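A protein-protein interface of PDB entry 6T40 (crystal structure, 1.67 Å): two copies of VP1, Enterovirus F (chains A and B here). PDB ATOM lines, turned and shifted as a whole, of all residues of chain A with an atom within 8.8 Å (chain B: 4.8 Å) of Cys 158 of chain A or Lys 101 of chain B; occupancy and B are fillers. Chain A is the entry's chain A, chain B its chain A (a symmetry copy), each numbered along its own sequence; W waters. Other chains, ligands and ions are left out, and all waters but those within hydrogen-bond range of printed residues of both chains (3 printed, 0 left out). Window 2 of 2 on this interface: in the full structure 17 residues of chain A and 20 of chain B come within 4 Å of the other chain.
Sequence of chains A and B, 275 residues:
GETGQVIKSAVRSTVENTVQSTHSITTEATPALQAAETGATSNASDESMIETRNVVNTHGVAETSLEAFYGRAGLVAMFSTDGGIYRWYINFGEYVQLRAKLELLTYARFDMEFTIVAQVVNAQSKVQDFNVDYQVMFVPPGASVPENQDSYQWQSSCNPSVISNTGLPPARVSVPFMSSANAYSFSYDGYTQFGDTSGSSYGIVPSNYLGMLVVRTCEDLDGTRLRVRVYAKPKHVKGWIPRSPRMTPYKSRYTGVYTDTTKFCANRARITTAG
OG of Ser 156 of chain A is in hydrogen-bond range of SD of Met 137 of chain A, 3.5 Å away.
The backbone NH of Phe 138 of chain A is in hydrogen-bond range of the backbone carbonyl oxygen of Pro 160 of chain A, 2.9 Å away.
The side-chain hydroxyl (OG) of Ser 156 of chain A sits at hydrogen-bond distance from the backbone carbonyl oxygen (O) of Asn 159 of chain A (2.6 Å).
OG of Ser 156 of chain A is in hydrogen-bond range of OG of Ser 161 of chain A (2.7 Å).
The side-chain sulfur (SG) of Cys 158 of chain A sits close to the side-chain hydroxyl (OG) of Ser 157 of chain A (3.7 Å).
The side-chain hydroxyl (OH) of Tyr 70 of chain B sits at hydrogen-bond distance from the backbone carbonyl oxygen (O) of Lys 101 of chain B, at 2.7 Å.
Water W2 lies within hydrogen-bond range of the backbone carbonyl oxygen of Gln 153 of chain A (2.8 Å), the side-chain amide nitrogen of Gln 97 of chain B (3.0 Å) and the side-chain amide oxygen of Asn 159 of chain A (3.2 Å).
Water W1 lies within hydrogen-bond range of O of Arg 72 of chain B (2.8 Å) and O of Ser 157 of chain A (2.9 Å).
Water W3 lies within hydrogen-bond range of OE1 of Gln 155 of chain A (2.9 Å) and N of Leu 98 of chain B (3.0 Å).
No position is printed for both chains.
Of the 14 printed residues of chain A, 5 touch a printed residue of chain B.
Hydrophobic or aromatic side chains of chain A that line the printed part of chain B: Pro 160.
Of the 12 printed residues of chain B, 4 touch a printed residue of chain A.
Printed residues of chain B that touch a printed residue of chain A: Arg 72, Gln 97, Leu 98 and Lys 101.
Phe 138 of chain A touches none of the printed residues of chain B.
Pro 140 of chain A touches none of the printed residues of chain B.
Of the printed residues of chain B, Gln 155 of chain A touches Gln 97 (3.2 Å).
Of the printed residues of chain B, Ser 156 of chain A touches Gln 97 (3.2 Å).
Of chain B, only Arg 72 and Lys 101 come within 4 Å of Cys 158 of chain A.
Ala 100 of chain B touches none of the printed residues of chain A.
The nearest printed residue of chain A that does not touch Leu 98 of chain B is Gln 155 of chain A (4.7 Å).
Ser 157 of chain A touches Arg 72 of chain B (O to CG, 3.6 Å).
Leu 98 of chain B touches Ser 157 of chain A.
Pro 160 of chain A touches Arg 72 of chain B.
The side-chain amide oxygen (OE1) of Gln 155 of chain A sits at hydrogen-bond distance from the backbone NH (N) of Gln 97 of chain B (3.2 Å).
The backbone NH of Ser 156 of chain A is in hydrogen-bond range of the side-chain amide oxygen of Gln 97 of chain B (3.2 Å).
N of Ser 157 of chain A sits at hydrogen-bond distance from OE1 of Gln 97 of chain B.
The backbone carbonyl oxygen (O) of Ser 157 of chain A sits at hydrogen-bond distance from the side-chain amino group (NZ) of Lys 101 of chain B.
The backbone carbonyl oxygen of Cys 158 of chain A sits at hydrogen-bond distance from the guanidinium group of Arg 72 of chain B (2.7 Å).
The side-chain sulfur (SG) of Cys 158 of chain A lies close to the side-chain amino group (NZ) of Lys 101 of chain B, 3.7 Å away.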
ATOM      1  N   MET A 137       7.258  25.856  -6.616  1.00  0.00           N
ATOM      2  CA  MET A 137       7.739  26.386  -7.880  1.00  0.00           C
ATOM      3  C   MET A 137       8.670  27.570  -7.678  1.00  0.00           C
ATOM      4  O   MET A 137       8.367  28.493  -6.921  1.00  0.00           O
ATOM      5  CB  MET A 137       6.555  26.798  -8.766  1.00  0.00           C
ATOM      6  CG  MET A 137       6.961  27.427 -10.097  1.00  0.00           C
ATOM      7  SD  MET A 137       5.579  27.627 -11.253  1.00  0.00           S
ATOM      8  CE  MET A 137       4.549  28.820 -10.364  1.00  0.00           C
ATOM      9  N   PHE A 138       9.816  27.524  -8.345  1.00  0.00           N
ATOM     10  CA  PHE A 138      10.782  28.610  -8.269  1.00  0.00           C
ATOM     11  C   PHE A 138      10.416  29.605  -9.364  1.00  0.00           C
ATOM     12  O   PHE A 138      10.433  29.269 -10.549  1.00  0.00           O
ATOM     13  CB  PHE A 138      12.203  28.078  -8.482  1.00  0.00           C
ATOM     14  CG  PHE A 138      13.236  29.156  -8.687  1.00  0.00           C
ATOM     15  CD1 PHE A 138      13.331  30.229  -7.803  1.00  0.00           C
ATOM     16  CD2 PHE A 138      14.121  29.093  -9.759  1.00  0.00           C
ATOM     17  CE1 PHE A 138      14.293  31.225  -7.985  1.00  0.00           C
ATOM     18  CE2 PHE A 138      15.088  30.083  -9.951  1.00  0.00           C
ATOM     19  CZ  PHE A 138      15.174  31.150  -9.062  1.00  0.00           C
ATOM     20  N   VAL A 139      10.064  30.821  -8.961  1.00  0.00           N
ATOM     21  CA  VAL A 139       9.691  31.863  -9.909  1.00  0.00           C
ATOM     22  C   VAL A 139      10.766  32.944  -9.925  1.00  0.00           C
ATOM     23  O   VAL A 139      10.859  33.751  -9.000  1.00  0.00           O
ATOM     24  CB  VAL A 139       8.340  32.516  -9.523  1.00  0.00           C
ATOM     25  CG1 VAL A 139       7.934  33.538 -10.581  1.00  0.00           C
ATOM     26  CG2 VAL A 139       7.267  31.445  -9.375  1.00  0.00           C
ATOM     27  N   PRO A 140      11.608  32.963 -10.971  1.00  0.00           N
ATOM     28  CA  PRO A 140      12.670  33.970 -11.066  1.00  0.00           C
ATOM     29  C   PRO A 140      12.066  35.361 -11.251  1.00  0.00           C
ATOM     30  O   PRO A 140      10.938  35.494 -11.733  1.00  0.00           O
ATOM     31  CB  PRO A 140      13.464  33.524 -12.296  1.00  0.00           C
ATOM     32  CG  PRO A 140      13.208  32.045 -12.364  1.00  0.00           C
ATOM     33  CD  PRO A 140      11.737  31.963 -12.045  1.00  0.00           C
ATOM     34  N   ALA A 143       9.201  36.764 -13.904  1.00  0.00           N
ATOM     35  CA  ALA A 143       8.198  35.771 -14.273  1.00  0.00           C
ATOM     36  C   ALA A 143       6.938  36.059 -13.462  1.00  0.00           C
ATOM     37  O   ALA A 143       7.012  36.595 -12.354  1.00  0.00           O
ATOM     38  CB  ALA A 143       8.709  34.359 -13.978  1.00  0.00           C
ATOM     39  N   GLN A 153       0.047  29.624 -14.082  1.00  0.00           N
ATOM     40  CA  GLN A 153       1.497  29.580 -13.895  1.00  0.00           C
ATOM     41  C   GLN A 153       1.987  28.254 -13.330  1.00  0.00           C
ATOM     42  O   GLN A 153       3.150  27.889 -13.513  1.00  0.00           O
ATOM     43  CB  GLN A 153       1.977  30.728 -12.994  1.00  0.00           C
ATOM     44  CG  GLN A 153       1.709  32.117 -13.565  1.00  0.00           C
ATOM     45  CD  GLN A 153       0.403  32.708 -13.067  1.00  0.00           C
ATOM     46  OE1 GLN A 153      -0.539  31.981 -12.754  1.00  0.00           O
ATOM     47  NE2 GLN A 153       0.338  34.032 -13.001  1.00  0.00           N
ATOM     48  N   TRP A 154       1.106  27.527 -12.651  1.00  0.00           N
ATOM     49  CA  TRP A 154       1.487  26.245 -12.073  1.00  0.00           C
ATOM     50  C   TRP A 154       1.809  25.193 -13.134  1.00  0.00           C
ATOM     51  O   TRP A 154       2.317  24.119 -12.809  1.00  0.00           O
ATOM     52  CB  TRP A 154       0.395  25.738 -11.125  1.00  0.00           C
ATOM     53  CG  TRP A 154       0.246  26.596  -9.894  1.00  0.00           C
ATOM     54  CD1 TRP A 154      -0.789  27.437  -9.596  1.00  0.00           C
ATOM     55  CD2 TRP A 154       1.166  26.689  -8.797  1.00  0.00           C
ATOM     56  NE1 TRP A 154      -0.572  28.047  -8.382  1.00  0.00           N
ATOM     57  CE2 TRP A 154       0.621  27.605  -7.870  1.00  0.00           C
ATOM     58  CE3 TRP A 154       2.399  26.086  -8.509  1.00  0.00           C
ATOM     59  CZ2 TRP A 154       1.265  27.933  -6.671  1.00  0.00           C
ATOM     60  CZ3 TRP A 154       3.042  26.411  -7.314  1.00  0.00           C
ATOM     61  CH2 TRP A 154       2.470  27.327  -6.411  1.00  0.00           C
ATOM     62  N   GLN A 155       1.511  25.495 -14.397  1.00  0.00           N
ATOM     63  CA  GLN A 155       1.834  24.578 -15.493  1.00  0.00           C
ATOM     64  C   GLN A 155       3.346  24.378 -15.449  1.00  0.00           C
ATOM     65  O   GLN A 155       3.865  23.328 -15.834  1.00  0.00           O
ATOM     66  CB  GLN A 155       1.440  25.190 -16.837  1.00  0.00           C
ATOM     67  CG  GLN A 155      -0.047  25.144 -17.125  1.00  0.00           C
ATOM     68  CD  GLN A 155      -0.412  25.950 -18.352  1.00  0.00           C
ATOM     69  OE1 GLN A 155       0.342  25.995 -19.325  1.00  0.00           O
ATOM     70  NE2 GLN A 155      -1.580  26.581 -18.319  1.00  0.00           N
ATOM     71  N   SER A 156       4.036  25.422 -14.998  1.00  0.00           N
ATOM     72  CA  SER A 156       5.486  25.423 -14.814  1.00  0.00           C
ATOM     73  C   SER A 156       6.305  24.828 -15.964  1.00  0.00           C
ATOM     74  O   SER A 156       7.226  24.049 -15.726  1.00  0.00           O
ATOM     75  CB  SER A 156       5.802  24.676 -13.511  1.00  0.00           C
ATOM     76  OG  SER A 156       7.069  25.029 -12.988  1.00  0.00           O
ATOM     77  N   SER A 157       5.997  25.212 -17.200  1.00  0.00           N
ATOM     78  CA  SER A 157       6.714  24.666 -18.355  1.00  0.00           C
ATOM     79  C   SER A 157       8.166  25.134 -18.458  1.00  0.00           C
ATOM     80  O   SER A 157       8.978  24.497 -19.132  1.00  0.00           O
ATOM     81  CB  SER A 157       5.987  25.016 -19.655  1.00  0.00           C
ATOM     82  OG  SER A 157       6.272  26.351 -20.047  1.00  0.00           O
ATOM     83  N   CYS A 158       8.486  26.254 -17.814  1.00  0.00           N
ATOM     84  CA  CYS A 158       9.850  26.780 -17.826  1.00  0.00           C
ATOM     85  C   CYS A 158      10.388  26.928 -16.409  1.00  0.00           C
ATOM     86  O   CYS A 158      11.538  26.581 -16.137  1.00  0.00           O
ATOM     87  CB  CYS A 158       9.906  28.129 -18.540  1.00  0.00           C
ATOM     88  SG  CYS A 158       9.590  28.018 -20.309  1.00  0.00           S
ATOM     89  N   ASN A 159       9.563  27.457 -15.508  1.00  0.00           N
ATOM     90  CA  ASN A 159       9.977  27.612 -14.114  1.00  0.00           C
ATOM     91  C   ASN A 159      10.235  26.219 -13.550  1.00  0.00           C
ATOM     92  O   ASN A 159       9.487  25.282 -13.832  1.00  0.00           O
ATOM     93  CB  ASN A 159       8.861  28.223 -13.254  1.00  0.00           C
ATOM     94  CG  ASN A 159       8.554  29.670 -13.589  1.00  0.00           C
ATOM     95  OD1 ASN A 159       7.546  30.210 -13.124  1.00  0.00           O
ATOM     96  ND2 ASN A 159       9.409  30.306 -14.375  1.00  0.00           N
ATOM     97  N   PRO A 160      11.302  26.057 -12.759  1.00  0.00           N
ATOM     98  CA  PRO A 160      11.536  24.724 -12.199  1.00  0.00           C
ATOM     99  C   PRO A 160      10.514  24.519 -11.073  1.00  0.00           C
ATOM    100  O   PRO A 160      10.192  25.460 -10.344  1.00  0.00           O
ATOM    101  CB  PRO A 160      12.956  24.822 -11.639  1.00  0.00           C
ATOM    102  CG  PRO A 160      13.594  25.895 -12.472  1.00  0.00           C
ATOM    103  CD  PRO A 160      12.490  26.914 -12.599  1.00  0.00           C
ATOM    104  N   SER A 161       9.996  23.304 -10.945  1.00  0.00           N
ATOM    105  CA  SER A 161       9.050  22.984  -9.881  1.00  0.00           C
ATOM    106  C   SER A 161       9.407  21.624  -9.321  1.00  0.00           C
ATOM    107  O   SER A 161       9.982  20.789 -10.015  1.00  0.00           O
ATOM    108  CB  SER A 161       7.605  22.901 -10.400  1.00  0.00           C
ATOM    109  OG  SER A 161       6.965  24.162 -10.447  1.00  0.00           O
ATOM    110  N   PHE B  69      16.583  24.336 -23.191  1.00  0.00           N
ATOM    111  CA  PHE B  69      15.355  25.120 -23.269  1.00  0.00           C
ATOM    112  C   PHE B  69      14.109  24.242 -23.124  1.00  0.00           C
ATOM    113  O   PHE B  69      13.193  24.565 -22.369  1.00  0.00           O
ATOM    114  CB  PHE B  69      15.305  25.857 -24.612  1.00  0.00           C
ATOM    115  CG  PHE B  69      14.147  26.809 -24.746  1.00  0.00           C
ATOM    116  CD1 PHE B  69      14.232  28.105 -24.245  1.00  0.00           C
ATOM    117  CD2 PHE B  69      12.975  26.412 -25.384  1.00  0.00           C
ATOM    118  CE1 PHE B  69      13.164  28.996 -24.377  1.00  0.00           C
ATOM    119  CE2 PHE B  69      11.900  27.291 -25.522  1.00  0.00           C
ATOM    120  CZ  PHE B  69      11.996  28.588 -25.018  1.00  0.00           C
ATOM    121  N   TYR B  70      14.092  23.125 -23.846  1.00  0.00           N
ATOM    122  CA  TYR B  70      12.949  22.213 -23.843  1.00  0.00           C
ATOM    123  C   TYR B  70      12.999  21.083 -22.827  1.00  0.00           C
ATOM    124  O   TYR B  70      11.960  20.547 -22.440  1.00  0.00           O
ATOM    125  CB  TYR B  70      12.791  21.591 -25.232  1.00  0.00           C
ATOM    126  CG  TYR B  70      12.327  22.558 -26.290  1.00  0.00           C
ATOM    127  CD1 TYR B  70      11.015  23.026 -26.301  1.00  0.00           C
ATOM    128  CD2 TYR B  70      13.201  23.010 -27.281  1.00  0.00           C
ATOM    129  CE1 TYR B  70      10.578  23.922 -27.273  1.00  0.00           C
ATOM    130  CE2 TYR B  70      12.774  23.910 -28.259  1.00  0.00           C
ATOM    131  CZ  TYR B  70      11.461  24.359 -28.245  1.00  0.00           C
ATOM    132  OH  TYR B  70      11.028  25.247 -29.199  1.00  0.00           O
ATOM    133  N   ARG B  72      12.634  20.066 -19.881  1.00  0.00           N
ATOM    134  CA  ARG B  72      12.028  20.055 -18.555  1.00  0.00           C
ATOM    135  C   ARG B  72      10.529  19.834 -18.712  1.00  0.00           C
ATOM    136  O   ARG B  72       9.948  20.166 -19.743  1.00  0.00           O
ATOM    137  CB  ARG B  72      12.335  21.348 -17.785  1.00  0.00           C
ATOM    138  CG  ARG B  72      11.938  22.639 -18.469  1.00  0.00           C
ATOM    139  CD  ARG B  72      12.451  23.829 -17.661  1.00  0.00           C
ATOM    140  NE  ARG B  72      13.913  23.861 -17.603  1.00  0.00           N
ATOM    141  CZ  ARG B  72      14.617  24.706 -16.852  1.00  0.00           C
ATOM    142  NH1 ARG B  72      14.001  25.599 -16.087  1.00  0.00           N
ATOM    143  NH2 ARG B  72      15.944  24.662 -16.866  1.00  0.00           N
ATOM    144  N   GLN B  97       1.583  27.284 -21.943  1.00  0.00           N
ATOM    145  CA  GLN B  97       3.019  27.448 -21.745  1.00  0.00           C
ATOM    146  C   GLN B  97       3.876  26.537 -22.619  1.00  0.00           C
ATOM    147  O   GLN B  97       4.726  27.024 -23.365  1.00  0.00           O
ATOM    148  CB  GLN B  97       3.390  27.283 -20.270  1.00  0.00           C
ATOM    149  CG  GLN B  97       2.779  28.357 -19.374  1.00  0.00           C
ATOM    150  CD  GLN B  97       3.433  28.413 -18.006  1.00  0.00           C
ATOM    151  OE1 GLN B  97       3.839  27.390 -17.464  1.00  0.00           O
ATOM    152  NE2 GLN B  97       3.525  29.611 -17.438  1.00  0.00           N
ATOM    153  N   LEU B  98       3.665  25.227 -22.547  1.00  0.00           N
ATOM    154  CA  LEU B  98       4.464  24.325 -23.372  1.00  0.00           C
ATOM    155  C   LEU B  98       4.148  24.542 -24.847  1.00  0.00           C
ATOM    156  O   LEU B  98       5.030  24.467 -25.703  1.00  0.00           O
ATOM    157  CB  LEU B  98       4.200  22.864 -22.998  1.00  0.00           C
ATOM    158  CG  LEU B  98       4.971  21.850 -23.854  1.00  0.00           C
ATOM    159  CD1 LEU B  98       6.467  22.142 -23.783  1.00  0.00           C
ATOM    160  CD2 LEU B  98       4.681  20.440 -23.373  1.00  0.00           C
ATOM    161  N   ARG B  99       2.883  24.819 -25.139  1.00  0.00           N
ATOM    162  CA  ARG B  99       2.451  25.050 -26.512  1.00  0.00           C
ATOM    163  C   ARG B  99       3.247  26.177 -27.171  1.00  0.00           C
ATOM    164  O   ARG B  99       3.759  26.022 -28.280  1.00  0.00           O
ATOM    165  CB  ARG B  99       0.961  25.393 -26.535  1.00  0.00           C
ATOM    166  CG  ARG B  99       0.409  25.649 -27.919  1.00  0.00           C
ATOM    167  CD  ARG B  99      -1.073  25.960 -27.843  1.00  0.00           C
ATOM    168  NE  ARG B  99      -1.645  26.230 -29.158  1.00  0.00           N
ATOM    169  CZ  ARG B  99      -2.942  26.407 -29.375  1.00  0.00           C
ATOM    170  NH1 ARG B  99      -3.797  26.335 -28.364  1.00  0.00           N
ATOM    171  NH2 ARG B  99      -3.382  26.670 -30.597  1.00  0.00           N
ATOM    172  N   ALA B 100       3.348  27.311 -26.484  1.00  0.00           N
ATOM    173  CA  ALA B 100       4.077  28.456 -27.023  1.00  0.00           C
ATOM    174  C   ALA B 100       5.556  28.134 -27.240  1.00  0.00           C
ATOM    175  O   ALA B 100       6.167  28.629 -28.188  1.00  0.00           O
ATOM    176  CB  ALA B 100       3.926  29.659 -26.092  1.00  0.00           C
ATOM    177  N   LYS B 101       6.130  27.311 -26.367  1.00  0.00           N
ATOM    178  CA  LYS B 101       7.537  26.930 -26.498  1.00  0.00           C
ATOM    179  C   LYS B 101       7.761  26.118 -27.769  1.00  0.00           C
ATOM    180  O   LYS B 101       8.679  26.393 -28.542  1.00  0.00           O
ATOM    181  CB  LYS B 101       7.993  26.086 -25.299  1.00  0.00           C
ATOM    182  CG  LYS B 101       8.012  26.817 -23.972  1.00  0.00           C
ATOM    183  CD  LYS B 101       8.504  25.910 -22.842  1.00  0.00           C
ATOM    184  CE  LYS B 101       9.994  25.609 -22.953  1.00  0.00           C
ATOM    185  NZ  LYS B 101      10.467  24.777 -21.803  1.00  0.00           N
ATOM    186  N   LEU B 102       6.923  25.111 -27.978  1.00  0.00           N
ATOM    187  CA  LEU B 102       7.057  24.256 -29.151  1.00  0.00           C
ATOM    188  C   LEU B 102       6.897  25.020 -30.460  1.00  0.00           C
ATOM    189  O   LEU B 102       7.576  24.724 -31.441  1.00  0.00           O
ATOM    190  CB  LEU B 102       6.035  23.116 -29.086  1.00  0.00           C
ATOM    191  CG  LEU B 102       6.243  22.131 -27.930  1.00  0.00           C
ATOM    192  CD1 LEU B 102       5.076  21.153 -27.871  1.00  0.00           C
ATOM    193  CD2 LEU B 102       7.562  21.393 -28.120  1.00  0.00           C
ATOM    194  N   GLU B 103       6.011  26.010 -30.475  1.00  0.00           N
ATOM    195  CA  GLU B 103       5.780  26.781 -31.689  1.00  0.00           C
ATOM    196  C   GLU B 103       6.923  27.719 -32.078  1.00  0.00           C
ATOM    197  O   GLU B 103       6.830  28.446 -33.066  1.00  0.00           O
ATOM    198  CB  GLU B 103       4.445  27.530 -31.580  1.00  0.00           C
ATOM    199  CG  GLU B 103       3.256  26.576 -31.740  1.00  0.00           C
ATOM    200  CD  GLU B 103       1.903  27.231 -31.527  1.00  0.00           C
ATOM    201  OE1 GLU B 103       1.819  28.476 -31.573  1.00  0.00           O
ATOM    202  OE2 GLU B 103       0.915  26.488 -31.326  1.00  0.00           O
ATOM    203  N   LEU B 104       8.010  27.685 -31.310  1.00  0.00           N
ATOM    204  CA  LEU B 104       9.186  28.496 -31.617  1.00  0.00           C
ATOM    205  C   LEU B 104      10.007  27.797 -32.707  1.00  0.00           C
ATOM    206  O   LEU B 104      10.957  28.366 -33.246  1.00  0.00           O
ATOM    207  CB  LEU B 104      10.049  28.690 -30.368  1.00  0.00           C
ATOM    208  CG  LEU B 104       9.456  29.593 -29.285  1.00  0.00           C
ATOM    209  CD1 LEU B 104      10.312  29.526 -28.024  1.00  0.00           C
ATOM    210  CD2 LEU B 104       9.374  31.022 -29.813  1.00  0.00           C
ATOM    211  N   LEU B 105       9.637  26.556 -33.014  1.00  0.00           N
ATOM    212  CA  LEU B 105      10.310  25.771 -34.049  1.00  0.00           C
ATOM    213  C   LEU B 105       9.269  25.308 -35.062  1.00  0.00           C
ATOM    214  O   LEU B 105       8.112  25.096 -34.710  1.00  0.00           O
ATOM    215  CB  LEU B 105      10.982  24.534 -33.443  1.00  0.00           C
ATOM    216  CG  LEU B 105      12.178  24.736 -32.508  1.00  0.00           C
ATOM    217  CD1 LEU B 105      12.576  23.398 -31.895  1.00  0.00           C
ATOM    218  CD2 LEU B 105      13.338  25.334 -33.286  1.00  0.00           C
HETATM  219  O   HOH W   1       8.060  22.111 -20.433  1.00  0.00           O
HETATM  220  O   HOH W   2       4.912  29.594 -14.777  1.00  0.00           O
HETATM  221  O   HOH W   3       2.091  23.954 -20.335  1.00  0.00           O
